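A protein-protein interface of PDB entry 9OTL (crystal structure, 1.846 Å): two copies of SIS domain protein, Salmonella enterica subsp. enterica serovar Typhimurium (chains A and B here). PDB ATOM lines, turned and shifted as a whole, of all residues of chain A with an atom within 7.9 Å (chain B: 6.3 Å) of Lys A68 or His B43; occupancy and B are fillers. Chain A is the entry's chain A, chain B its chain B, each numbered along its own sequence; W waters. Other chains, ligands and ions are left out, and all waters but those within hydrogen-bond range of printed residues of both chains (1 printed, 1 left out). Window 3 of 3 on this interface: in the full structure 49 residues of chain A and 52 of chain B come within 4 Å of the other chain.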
ATOM      1  N   LEU A  63     -20.030  14.333 -18.994  1.00  0.00           N
ATOM      2  CA  LEU A  63     -20.185  14.730 -20.375  1.00  0.00           C
ATOM      3  C   LEU A  63     -19.034  15.645 -20.834  1.00  0.00           C
ATOM      4  O   LEU A  63     -18.584  15.578 -21.981  1.00  0.00           O
ATOM      5  CB  LEU A  63     -21.539  15.379 -20.593  1.00  0.00           C
ATOM      6  CG  LEU A  63     -22.724  14.424 -20.500  1.00  0.00           C
ATOM      7  CD1 LEU A  63     -24.043  15.216 -20.611  1.00  0.00           C
ATOM      8  CD2 LEU A  63     -22.641  13.311 -21.551  1.00  0.00           C
ATOM      9  N   GLU A  64     -18.494  16.483 -19.971  1.00  0.00           N
ATOM     10  CA  GLU A  64     -17.435  17.384 -20.432  1.00  0.00           C
ATOM     11  C   GLU A  64     -16.149  16.596 -20.688  1.00  0.00           C
ATOM     12  O   GLU A  64     -15.416  16.962 -21.607  1.00  0.00           O
ATOM     13  CB  GLU A  64     -17.398  18.703 -19.678  1.00  0.00           C
ATOM     14  CG  GLU A  64     -17.063  18.606 -18.206  1.00  0.00           C
ATOM     15  CD  GLU A  64     -17.301  19.926 -17.476  1.00  0.00           C
ATOM     16  OE1 GLU A  64     -17.805  20.879 -18.134  1.00  0.00           O
ATOM     17  OE2 GLU A  64     -16.957  20.019 -16.259  1.00  0.00           O
ATOM     18  N   LYS A  65     -15.952  15.483 -19.957  1.00  0.00           N
ATOM     19  CA  LYS A  65     -14.777  14.637 -20.141  1.00  0.00           C
ATOM     20  C   LYS A  65     -14.930  13.729 -21.356  1.00  0.00           C
ATOM     21  O   LYS A  65     -13.958  13.523 -22.083  1.00  0.00           O
ATOM     22  CB  LYS A  65     -14.469  13.825 -18.886  1.00  0.00           C
ATOM     23  CG  LYS A  65     -13.405  12.717 -18.997  1.00  0.00           C
ATOM     24  CD  LYS A  65     -11.974  13.200 -19.155  1.00  0.00           C
ATOM     25  CE  LYS A  65     -11.088  12.057 -19.501  1.00  0.00           C
ATOM     26  NZ  LYS A  65      -9.713  12.548 -19.431  1.00  0.00           N
ATOM     27  N   GLU A  66     -16.145  13.190 -21.575  1.00  0.00           N
ATOM     28  CA  GLU A  66     -16.327  12.009 -22.388  1.00  0.00           C
ATOM     29  C   GLU A  66     -16.994  12.253 -23.740  1.00  0.00           C
ATOM     30  O   GLU A  66     -16.855  11.406 -24.611  1.00  0.00           O
ATOM     31  CB  GLU A  66     -17.215  11.001 -21.674  1.00  0.00           C
ATOM     32  CG  GLU A  66     -16.654  10.528 -20.343  1.00  0.00           C
ATOM     33  CD  GLU A  66     -15.430   9.661 -20.360  1.00  0.00           C
ATOM     34  OE1 GLU A  66     -14.997   9.370 -19.219  1.00  0.00           O
ATOM     35  OE2 GLU A  66     -14.965   9.255 -21.431  1.00  0.00           O
ATOM     36  N   ALA A  67     -17.727  13.350 -23.911  1.00  0.00           N
ATOM     37  CA  ALA A  67     -18.532  13.579 -25.100  1.00  0.00           C
ATOM     38  C   ALA A  67     -17.742  14.318 -26.188  1.00  0.00           C
ATOM     39  O   ALA A  67     -17.042  15.286 -25.928  1.00  0.00           O
ATOM     40  CB  ALA A  67     -19.754  14.374 -24.748  1.00  0.00           C
ATOM     41  N   LYS A  68     -17.901  13.888 -27.436  1.00  0.00           N
ATOM     42  CA  LYS A  68     -17.341  14.617 -28.556  1.00  0.00           C
ATOM     43  C   LYS A  68     -18.376  15.464 -29.275  1.00  0.00           C
ATOM     44  O   LYS A  68     -18.024  16.420 -29.949  1.00  0.00           O
ATOM     45  CB  LYS A  68     -16.678  13.596 -29.476  1.00  0.00           C
ATOM     46  CG  LYS A  68     -15.422  12.979 -28.855  1.00  0.00           C
ATOM     47  CD  LYS A  68     -14.634  12.005 -29.727  1.00  0.00           C
ATOM     48  CE  LYS A  68     -15.415  10.904 -30.378  1.00  0.00           C
ATOM     49  NZ  LYS A  68     -15.936   9.845 -29.499  1.00  0.00           N
ATOM     50  N   ALA A  69     -19.655  15.126 -29.167  1.00  0.00           N
ATOM     51  CA  ALA A  69     -20.661  15.779 -29.997  1.00  0.00           C
ATOM     52  C   ALA A  69     -21.814  16.373 -29.174  1.00  0.00           C
ATOM     53  O   ALA A  69     -22.643  17.107 -29.704  1.00  0.00           O
ATOM     54  CB  ALA A  69     -21.161  14.776 -31.033  1.00  0.00           C
ATOM     55  N   LEU A  70     -21.896  16.053 -27.886  1.00  0.00           N
ATOM     56  CA  LEU A  70     -22.974  16.535 -27.032  1.00  0.00           C
ATOM     57  C   LEU A  70     -22.468  17.691 -26.168  1.00  0.00           C
ATOM     58  O   LEU A  70     -21.364  17.609 -25.651  1.00  0.00           O
ATOM     59  CB  LEU A  70     -23.301  15.283 -26.230  1.00  0.00           C
ATOM     60  CG  LEU A  70     -24.766  14.970 -26.000  1.00  0.00           C
ATOM     61  CD1 LEU A  70     -25.603  14.836 -27.266  1.00  0.00           C
ATOM     62  CD2 LEU A  70     -24.780  13.675 -25.182  1.00  0.00           C
ATOM     63  N   THR A  71     -23.215  18.799 -26.078  1.00  0.00           N
ATOM     64  CA  THR A  71     -22.885  19.853 -25.128  1.00  0.00           C
ATOM     65  C   THR A  71     -23.593  19.559 -23.807  1.00  0.00           C
ATOM     66  O   THR A  71     -24.623  18.881 -23.793  1.00  0.00           O
ATOM     67  CB  THR A  71     -23.258  21.235 -25.658  1.00  0.00           C
ATOM     68  OG1 THR A  71     -24.660  21.407 -25.524  1.00  0.00           O
ATOM     69  CG2 THR A  71     -22.894  21.443 -27.116  1.00  0.00           C
ATOM     70  N   LEU A 165     -25.155   9.576 -23.799  1.00  0.00           N
ATOM     71  CA  LEU A 165     -23.958   9.547 -24.615  1.00  0.00           C
ATOM     72  C   LEU A 165     -23.938   8.250 -25.440  1.00  0.00           C
ATOM     73  O   LEU A 165     -23.667   8.245 -26.643  1.00  0.00           O
ATOM     74  CB  LEU A 165     -22.733   9.702 -23.721  1.00  0.00           C
ATOM     75  CG  LEU A 165     -21.380   9.652 -24.447  1.00  0.00           C
ATOM     76  CD1 LEU A 165     -21.165  10.927 -25.265  1.00  0.00           C
ATOM     77  CD2 LEU A 165     -20.238   9.431 -23.471  1.00  0.00           C
ATOM     78  N   GLU A 169     -23.858   8.727 -29.515  1.00  0.00           N
ATOM     79  CA  GLU A 169     -22.507   8.862 -30.006  1.00  0.00           C
ATOM     80  C   GLU A 169     -21.738   7.573 -29.749  1.00  0.00           C
ATOM     81  O   GLU A 169     -20.715   7.316 -30.368  1.00  0.00           O
ATOM     82  CB  GLU A 169     -22.074  10.070 -29.173  1.00  0.00           C
ATOM     83  CG  GLU A 169     -20.611  10.455 -29.263  1.00  0.00           C
ATOM     84  CD  GLU A 169     -20.258  11.712 -28.482  1.00  0.00           C
ATOM     85  OE1 GLU A 169     -21.053  12.642 -28.320  1.00  0.00           O
ATOM     86  OE2 GLU A 169     -19.086  11.771 -28.065  1.00  0.00           O
ATOM     87  N   GLY A 170     -22.221   6.763 -28.807  1.00  0.00           N
ATOM     88  CA  GLY A 170     -21.457   5.626 -28.330  1.00  0.00           C
ATOM     89  C   GLY A 170     -20.560   6.019 -27.158  1.00  0.00           C
ATOM     90  O   GLY A 170     -20.103   7.141 -27.041  1.00  0.00           O
ATOM     91  N   TYR A 171     -20.383   5.106 -26.225  1.00  0.00           N
ATOM     92  CA  TYR A 171     -19.477   5.343 -25.132  1.00  0.00           C
ATOM     93  C   TYR A 171     -18.612   4.115 -24.937  1.00  0.00           C
ATOM     94  O   TYR A 171     -19.123   3.085 -24.545  1.00  0.00           O
ATOM     95  CB  TYR A 171     -20.339   5.674 -23.901  1.00  0.00           C
ATOM     96  CG  TYR A 171     -19.603   5.682 -22.573  1.00  0.00           C
ATOM     97  CD1 TYR A 171     -18.370   6.301 -22.450  1.00  0.00           C
ATOM     98  CD2 TYR A 171     -20.181   5.149 -21.430  1.00  0.00           C
ATOM     99  CE1 TYR A 171     -17.740   6.384 -21.226  1.00  0.00           C
ATOM    100  CE2 TYR A 171     -19.561   5.224 -20.193  1.00  0.00           C
ATOM    101  CZ  TYR A 171     -18.304   5.792 -20.106  1.00  0.00           C
ATOM    102  OH  TYR A 171     -17.649   5.816 -18.908  1.00  0.00           O
ATOM    103  N   ALA A 172     -17.307   4.311 -24.985  1.00  0.00           N
ATOM    104  CA  ALA A 172     -16.339   3.228 -24.963  1.00  0.00           C
ATOM    105  C   ALA A 172     -16.354   2.448 -23.652  1.00  0.00           C
ATOM    106  O   ALA A 172     -15.929   1.302 -23.649  1.00  0.00           O
ATOM    107  CB  ALA A 172     -14.957   3.805 -25.208  1.00  0.00           C
ATOM    108  N   GLY B  40     -13.762  21.540 -38.729  1.00  0.00           N
ATOM    109  CA  GLY B  40     -14.144  22.822 -38.170  1.00  0.00           C
ATOM    110  C   GLY B  40     -13.875  22.887 -36.658  1.00  0.00           C
ATOM    111  O   GLY B  40     -13.493  21.901 -36.033  1.00  0.00           O
ATOM    112  N   VAL B  41     -14.006  24.090 -36.111  1.00  0.00           N
ATOM    113  CA  VAL B  41     -13.942  24.325 -34.674  1.00  0.00           C
ATOM    114  C   VAL B  41     -15.287  23.984 -34.043  1.00  0.00           C
ATOM    115  O   VAL B  41     -16.306  24.590 -34.374  1.00  0.00           O
ATOM    116  CB  VAL B  41     -13.602  25.795 -34.423  1.00  0.00           C
ATOM    117  CG1 VAL B  41     -13.401  26.058 -32.919  1.00  0.00           C
ATOM    118  CG2 VAL B  41     -12.374  26.194 -35.232  1.00  0.00           C
ATOM    119  N   LYS B  42     -15.289  22.983 -33.168  1.00  0.00           N
ATOM    120  CA  LYS B  42     -16.494  22.606 -32.461  1.00  0.00           C
ATOM    121  C   LYS B  42     -16.366  22.837 -30.954  1.00  0.00           C
ATOM    122  O   LYS B  42     -17.372  22.752 -30.244  1.00  0.00           O
ATOM    123  CB  LYS B  42     -16.717  21.113 -32.701  1.00  0.00           C
ATOM    124  CG  LYS B  42     -16.853  20.698 -34.177  1.00  0.00           C
ATOM    125  CD  LYS B  42     -16.813  19.176 -34.299  1.00  0.00           C
ATOM    126  CE  LYS B  42     -17.129  18.683 -35.657  1.00  0.00           C
ATOM    127  NZ  LYS B  42     -17.110  17.226 -35.640  1.00  0.00           N
ATOM    128  N   HIS B  43     -15.146  23.086 -30.443  1.00  0.00           N
ATOM    129  CA  HIS B  43     -14.931  23.099 -28.997  1.00  0.00           C
ATOM    130  C   HIS B  43     -13.914  24.188 -28.666  1.00  0.00           C
ATOM    131  O   HIS B  43     -12.895  24.315 -29.346  1.00  0.00           O
ATOM    132  CB  HIS B  43     -14.410  21.761 -28.440  1.00  0.00           C
ATOM    133  CG  HIS B  43     -15.155  20.553 -28.895  1.00  0.00           C
ATOM    134  ND1 HIS B  43     -14.732  19.674 -29.881  1.00  0.00           N
ATOM    135  CD2 HIS B  43     -16.353  20.088 -28.478  1.00  0.00           C
ATOM    136  CE1 HIS B  43     -15.657  18.735 -30.050  1.00  0.00           C
ATOM    137  NE2 HIS B  43     -16.640  18.968 -29.212  1.00  0.00           N
ATOM    138  N   VAL B  44     -14.199  24.963 -27.616  1.00  0.00           N
ATOM    139  CA  VAL B  44     -13.309  26.008 -27.158  1.00  0.00           C
ATOM    140  C   VAL B  44     -13.013  25.737 -25.688  1.00  0.00           C
ATOM    141  O   VAL B  44     -13.943  25.557 -24.872  1.00  0.00           O
ATOM    142  CB  VAL B  44     -13.955  27.405 -27.340  1.00  0.00           C
ATOM    143  CG1 VAL B  44     -12.978  28.529 -27.035  1.00  0.00           C
ATOM    144  CG2 VAL B  44     -14.568  27.535 -28.697  1.00  0.00           C
ATOM    145  N   TYR B  45     -11.718  25.739 -25.358  1.00  0.00           N
ATOM    146  CA  TYR B  45     -11.293  25.502 -23.997  1.00  0.00           C
ATOM    147  C   TYR B  45     -10.526  26.727 -23.538  1.00  0.00           C
ATOM    148  O   TYR B  45      -9.577  27.092 -24.203  1.00  0.00           O
ATOM    149  CB  TYR B  45     -10.448  24.229 -23.841  1.00  0.00           C
ATOM    150  CG  TYR B  45     -11.278  23.002 -24.166  1.00  0.00           C
ATOM    151  CD1 TYR B  45     -12.309  22.575 -23.332  1.00  0.00           C
ATOM    152  CD2 TYR B  45     -11.015  22.248 -25.310  1.00  0.00           C
ATOM    153  CE1 TYR B  45     -13.106  21.504 -23.691  1.00  0.00           C
ATOM    154  CE2 TYR B  45     -11.771  21.143 -25.646  1.00  0.00           C
ATOM    155  CZ  TYR B  45     -12.833  20.784 -24.840  1.00  0.00           C
ATOM    156  OH  TYR B  45     -13.547  19.680 -25.196  1.00  0.00           O
ATOM    157  N   ALA B  69     -23.586  25.537 -31.737  1.00  0.00           N
ATOM    158  CA  ALA B  69     -22.772  24.477 -32.312  1.00  0.00           C
ATOM    159  C   ALA B  69     -21.303  24.605 -31.907  1.00  0.00           C
ATOM    160  O   ALA B  69     -20.382  24.188 -32.623  1.00  0.00           O
ATOM    161  CB  ALA B  69     -22.913  24.529 -33.821  1.00  0.00           C
ATOM    162  N   LEU B  70     -21.074  25.198 -30.748  1.00  0.00           N
ATOM    163  CA  LEU B  70     -19.757  25.264 -30.141  1.00  0.00           C
ATOM    164  C   LEU B  70     -19.946  24.930 -28.659  1.00  0.00           C
ATOM    165  O   LEU B  70     -20.903  25.418 -28.048  1.00  0.00           O
ATOM    166  CB  LEU B  70     -19.418  26.731 -30.403  1.00  0.00           C
ATOM    167  CG  LEU B  70     -17.971  27.150 -30.630  1.00  0.00           C
ATOM    168  CD1 LEU B  70     -17.309  26.381 -31.765  1.00  0.00           C
ATOM    169  CD2 LEU B  70     -17.981  28.658 -30.934  1.00  0.00           C
ATOM    170  N   THR B  71     -19.095  24.059 -28.119  1.00  0.00           N
ATOM    171  CA  THR B  71     -19.041  23.804 -26.700  1.00  0.00           C
ATOM    172  C   THR B  71     -17.941  24.694 -26.130  1.00  0.00           C
ATOM    173  O   THR B  71     -17.035  25.067 -26.848  1.00  0.00           O
ATOM    174  CB  THR B  71     -18.719  22.331 -26.434  1.00  0.00           C
ATOM    175  OG1 THR B  71     -17.333  22.230 -26.740  1.00  0.00           O
ATOM    176  CG2 THR B  71     -19.509  21.355 -27.295  1.00  0.00           C
ATOM    177  N   VAL B  72     -18.021  24.987 -24.832  1.00  0.00           N
ATOM    178  CA  VAL B  72     -17.015  25.745 -24.147  1.00  0.00           C
ATOM    179  C   VAL B  72     -16.746  25.001 -22.853  1.00  0.00           C
ATOM    180  O   VAL B  72     -17.688  24.553 -22.220  1.00  0.00           O
ATOM    181  CB  VAL B  72     -17.402  27.220 -23.873  1.00  0.00           C
ATOM    182  CG1 VAL B  72     -18.627  27.402 -22.981  1.00  0.00           C
ATOM    183  CG2 VAL B  72     -16.257  28.011 -23.305  1.00  0.00           C
ATOM    184  N   VAL B  86     -11.813  14.402 -23.807  1.00  0.00           N
ATOM    185  CA  VAL B  86     -11.643  13.571 -24.978  1.00  0.00           C
ATOM    186  C   VAL B  86     -11.811  14.377 -26.273  1.00  0.00           C
ATOM    187  O   VAL B  86     -11.329  13.916 -27.303  1.00  0.00           O
ATOM    188  CB  VAL B  86     -12.643  12.403 -24.913  1.00  0.00           C
ATOM    189  CG1 VAL B  86     -12.674  11.635 -26.228  1.00  0.00           C
ATOM    190  CG2 VAL B  86     -12.338  11.493 -23.720  1.00  0.00           C
ATOM    191  N   ALA B  87     -12.590  15.480 -26.255  1.00  0.00           N
ATOM    192  CA  ALA B  87     -12.803  16.306 -27.428  1.00  0.00           C
ATOM    193  C   ALA B  87     -11.551  17.130 -27.768  1.00  0.00           C
ATOM    194  O   ALA B  87     -11.549  17.828 -28.760  1.00  0.00           O
ATOM    195  CB  ALA B  87     -13.984  17.200 -27.221  1.00  0.00           C
ATOM    196  N   LEU B  88     -10.533  17.121 -26.913  1.00  0.00           N
ATOM    197  CA  LEU B  88      -9.309  17.830 -27.204  1.00  0.00           C
ATOM    198  C   LEU B  88      -8.633  17.210 -28.431  1.00  0.00           C
ATOM    199  O   LEU B  88      -8.185  16.068 -28.391  1.00  0.00           O
ATOM    200  CB  LEU B  88      -8.345  17.841 -26.039  1.00  0.00           C
ATOM    201  CG  LEU B  88      -7.049  18.629 -26.246  1.00  0.00           C
ATOM    202  CD1 LEU B  88      -7.331  20.076 -26.461  1.00  0.00           C
ATOM    203  CD2 LEU B  88      -6.133  18.434 -25.062  1.00  0.00           C
ATOM    204  N   ASN B  91     -10.557  19.556 -33.708  1.00  0.00           N
ATOM    205  CA  ASN B  91     -11.745  20.421 -33.732  1.00  0.00           C
ATOM    206  C   ASN B  91     -11.895  21.277 -32.472  1.00  0.00           C
ATOM    207  O   ASN B  91     -12.950  21.855 -32.272  1.00  0.00           O
ATOM    208  CB  ASN B  91     -12.997  19.584 -33.940  1.00  0.00           C
ATOM    209  CG  ASN B  91     -12.864  18.682 -35.152  1.00  0.00           C
ATOM    210  OD1 ASN B  91     -12.812  17.448 -35.007  1.00  0.00           O
ATOM    211  ND2 ASN B  91     -12.795  19.277 -36.345  1.00  0.00           N
ATOM    212  N   ALA B  92     -10.850  21.345 -31.630  1.00  0.00           N
ATOM    213  CA  ALA B  92     -10.810  22.166 -30.424  1.00  0.00           C
ATOM    214  C   ALA B  92      -9.852  23.325 -30.622  1.00  0.00           C
ATOM    215  O   ALA B  92      -8.794  23.156 -31.238  1.00  0.00           O
ATOM    216  CB  ALA B  92     -10.344  21.355 -29.210  1.00  0.00           C
ATOM    217  N   VAL B  93     -10.203  24.486 -30.069  1.00  0.00           N
ATOM    218  CA  VAL B  93      -9.247  25.562 -29.863  1.00  0.00           C
ATOM    219  C   VAL B  93      -8.980  25.725 -28.380  1.00  0.00           C
ATOM    220  O   VAL B  93      -9.930  25.739 -27.597  1.00  0.00           O
ATOM    221  CB  VAL B  93      -9.851  26.837 -30.466  1.00  0.00           C
ATOM    222  CG1 VAL B  93      -8.939  28.038 -30.247  1.00  0.00           C
ATOM    223  CG2 VAL B  93     -10.135  26.610 -31.950  1.00  0.00           C
ATOM    224  N   VAL B  94      -7.719  25.952 -28.003  1.00  0.00           N
ATOM    225  CA  VAL B  94      -7.393  26.142 -26.616  1.00  0.00           C
ATOM    226  C   VAL B  94      -6.815  27.520 -26.457  1.00  0.00           C
ATOM    227  O   VAL B  94      -5.904  27.900 -27.225  1.00  0.00           O
ATOM    228  CB  VAL B  94      -6.431  25.044 -26.157  1.00  0.00           C
ATOM    229  CG1 VAL B  94      -6.115  25.187 -24.687  1.00  0.00           C
ATOM    230  CG2 VAL B  94      -7.009  23.662 -26.434  1.00  0.00           C
HETATM  231  O   HOH W   1     -15.466  18.978 -23.467  1.00  0.00           O
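The backbone carbonyl oxygen (O) of Lys A65 is in hydrogen-bond range of the backbone NH (N) of Val B86 (2.9 Å). NE2 of His B43 sits at hydrogen-bond distance from O of Lys A68, 3.0 Å away.
NZ of Lys A68 is in salt-bridge range of OE2 of Glu A169. The backbone NH (N) of Thr B71 lies within hydrogen-bond range of the backbone carbonyl oxygen (O) of Lys B42, at 3.0 Å. The backbone NH (N) of His B43 lies within hydrogen-bond range of the backbone carbonyl oxygen (O) of Asn B91 (3.1 Å). The backbone carbonyl oxygen of His B43 sits at hydrogen-bond distance from the backbone NH of Val B93. The backbone NH (N) of Val B44 lies within hydrogen-bond range of the backbone carbonyl oxygen (O) of Thr B71.
Among the printed residues, merely in contact across the chains: Ala A67 with Ala B87 (3.8 Å) and Thr A71 with Thr B71 (3.4 Å).
Of the printed residues of chain B, Lys A65 touches Val B86 (2.9 Å). Of the printed residues of chain B, Ala A67 touches Ala B87 (3.8 Å). Of chain B, only His B43 (3.0 Å) comes within 4 Å of Lys A68. Of the printed residues of chain B, Thr A71 touches Thr B71. Ala A172 touches none of the printed residues of chain B. His B43 touches just one residue of chain A: Lys A68 (3.0 Å). Val B44 touches none of the printed residues of chain A. Of the printed residues of chain A, Val B86 touches Lys A65. Printed residues of chain A within 4 Å of Ala B87: Ala A67. The nearest residue of chain A that does not touch His B43 is Ala A69 (4.9 Å). The nearest printed residue of chain A that does not touch Thr B71 is Leu A70 (4.5 Å).
Printed residues of chain A that touch a printed residue of chain B: Lys A65, Ala A67, Lys A68 and Thr A71. Of the 17 printed residues of chain B, 4 touch a printed residue of chain A. Among the printed residues, 4 pairs touch across the chains.
Thr B71 touches its own counterpart, Thr A71. 3 positions are printed for both chains.
Water W1 lies within hydrogen-bond range of the side-chain hydroxyl of Tyr B45 and the backbone carbonyl oxygen of Glu A64.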
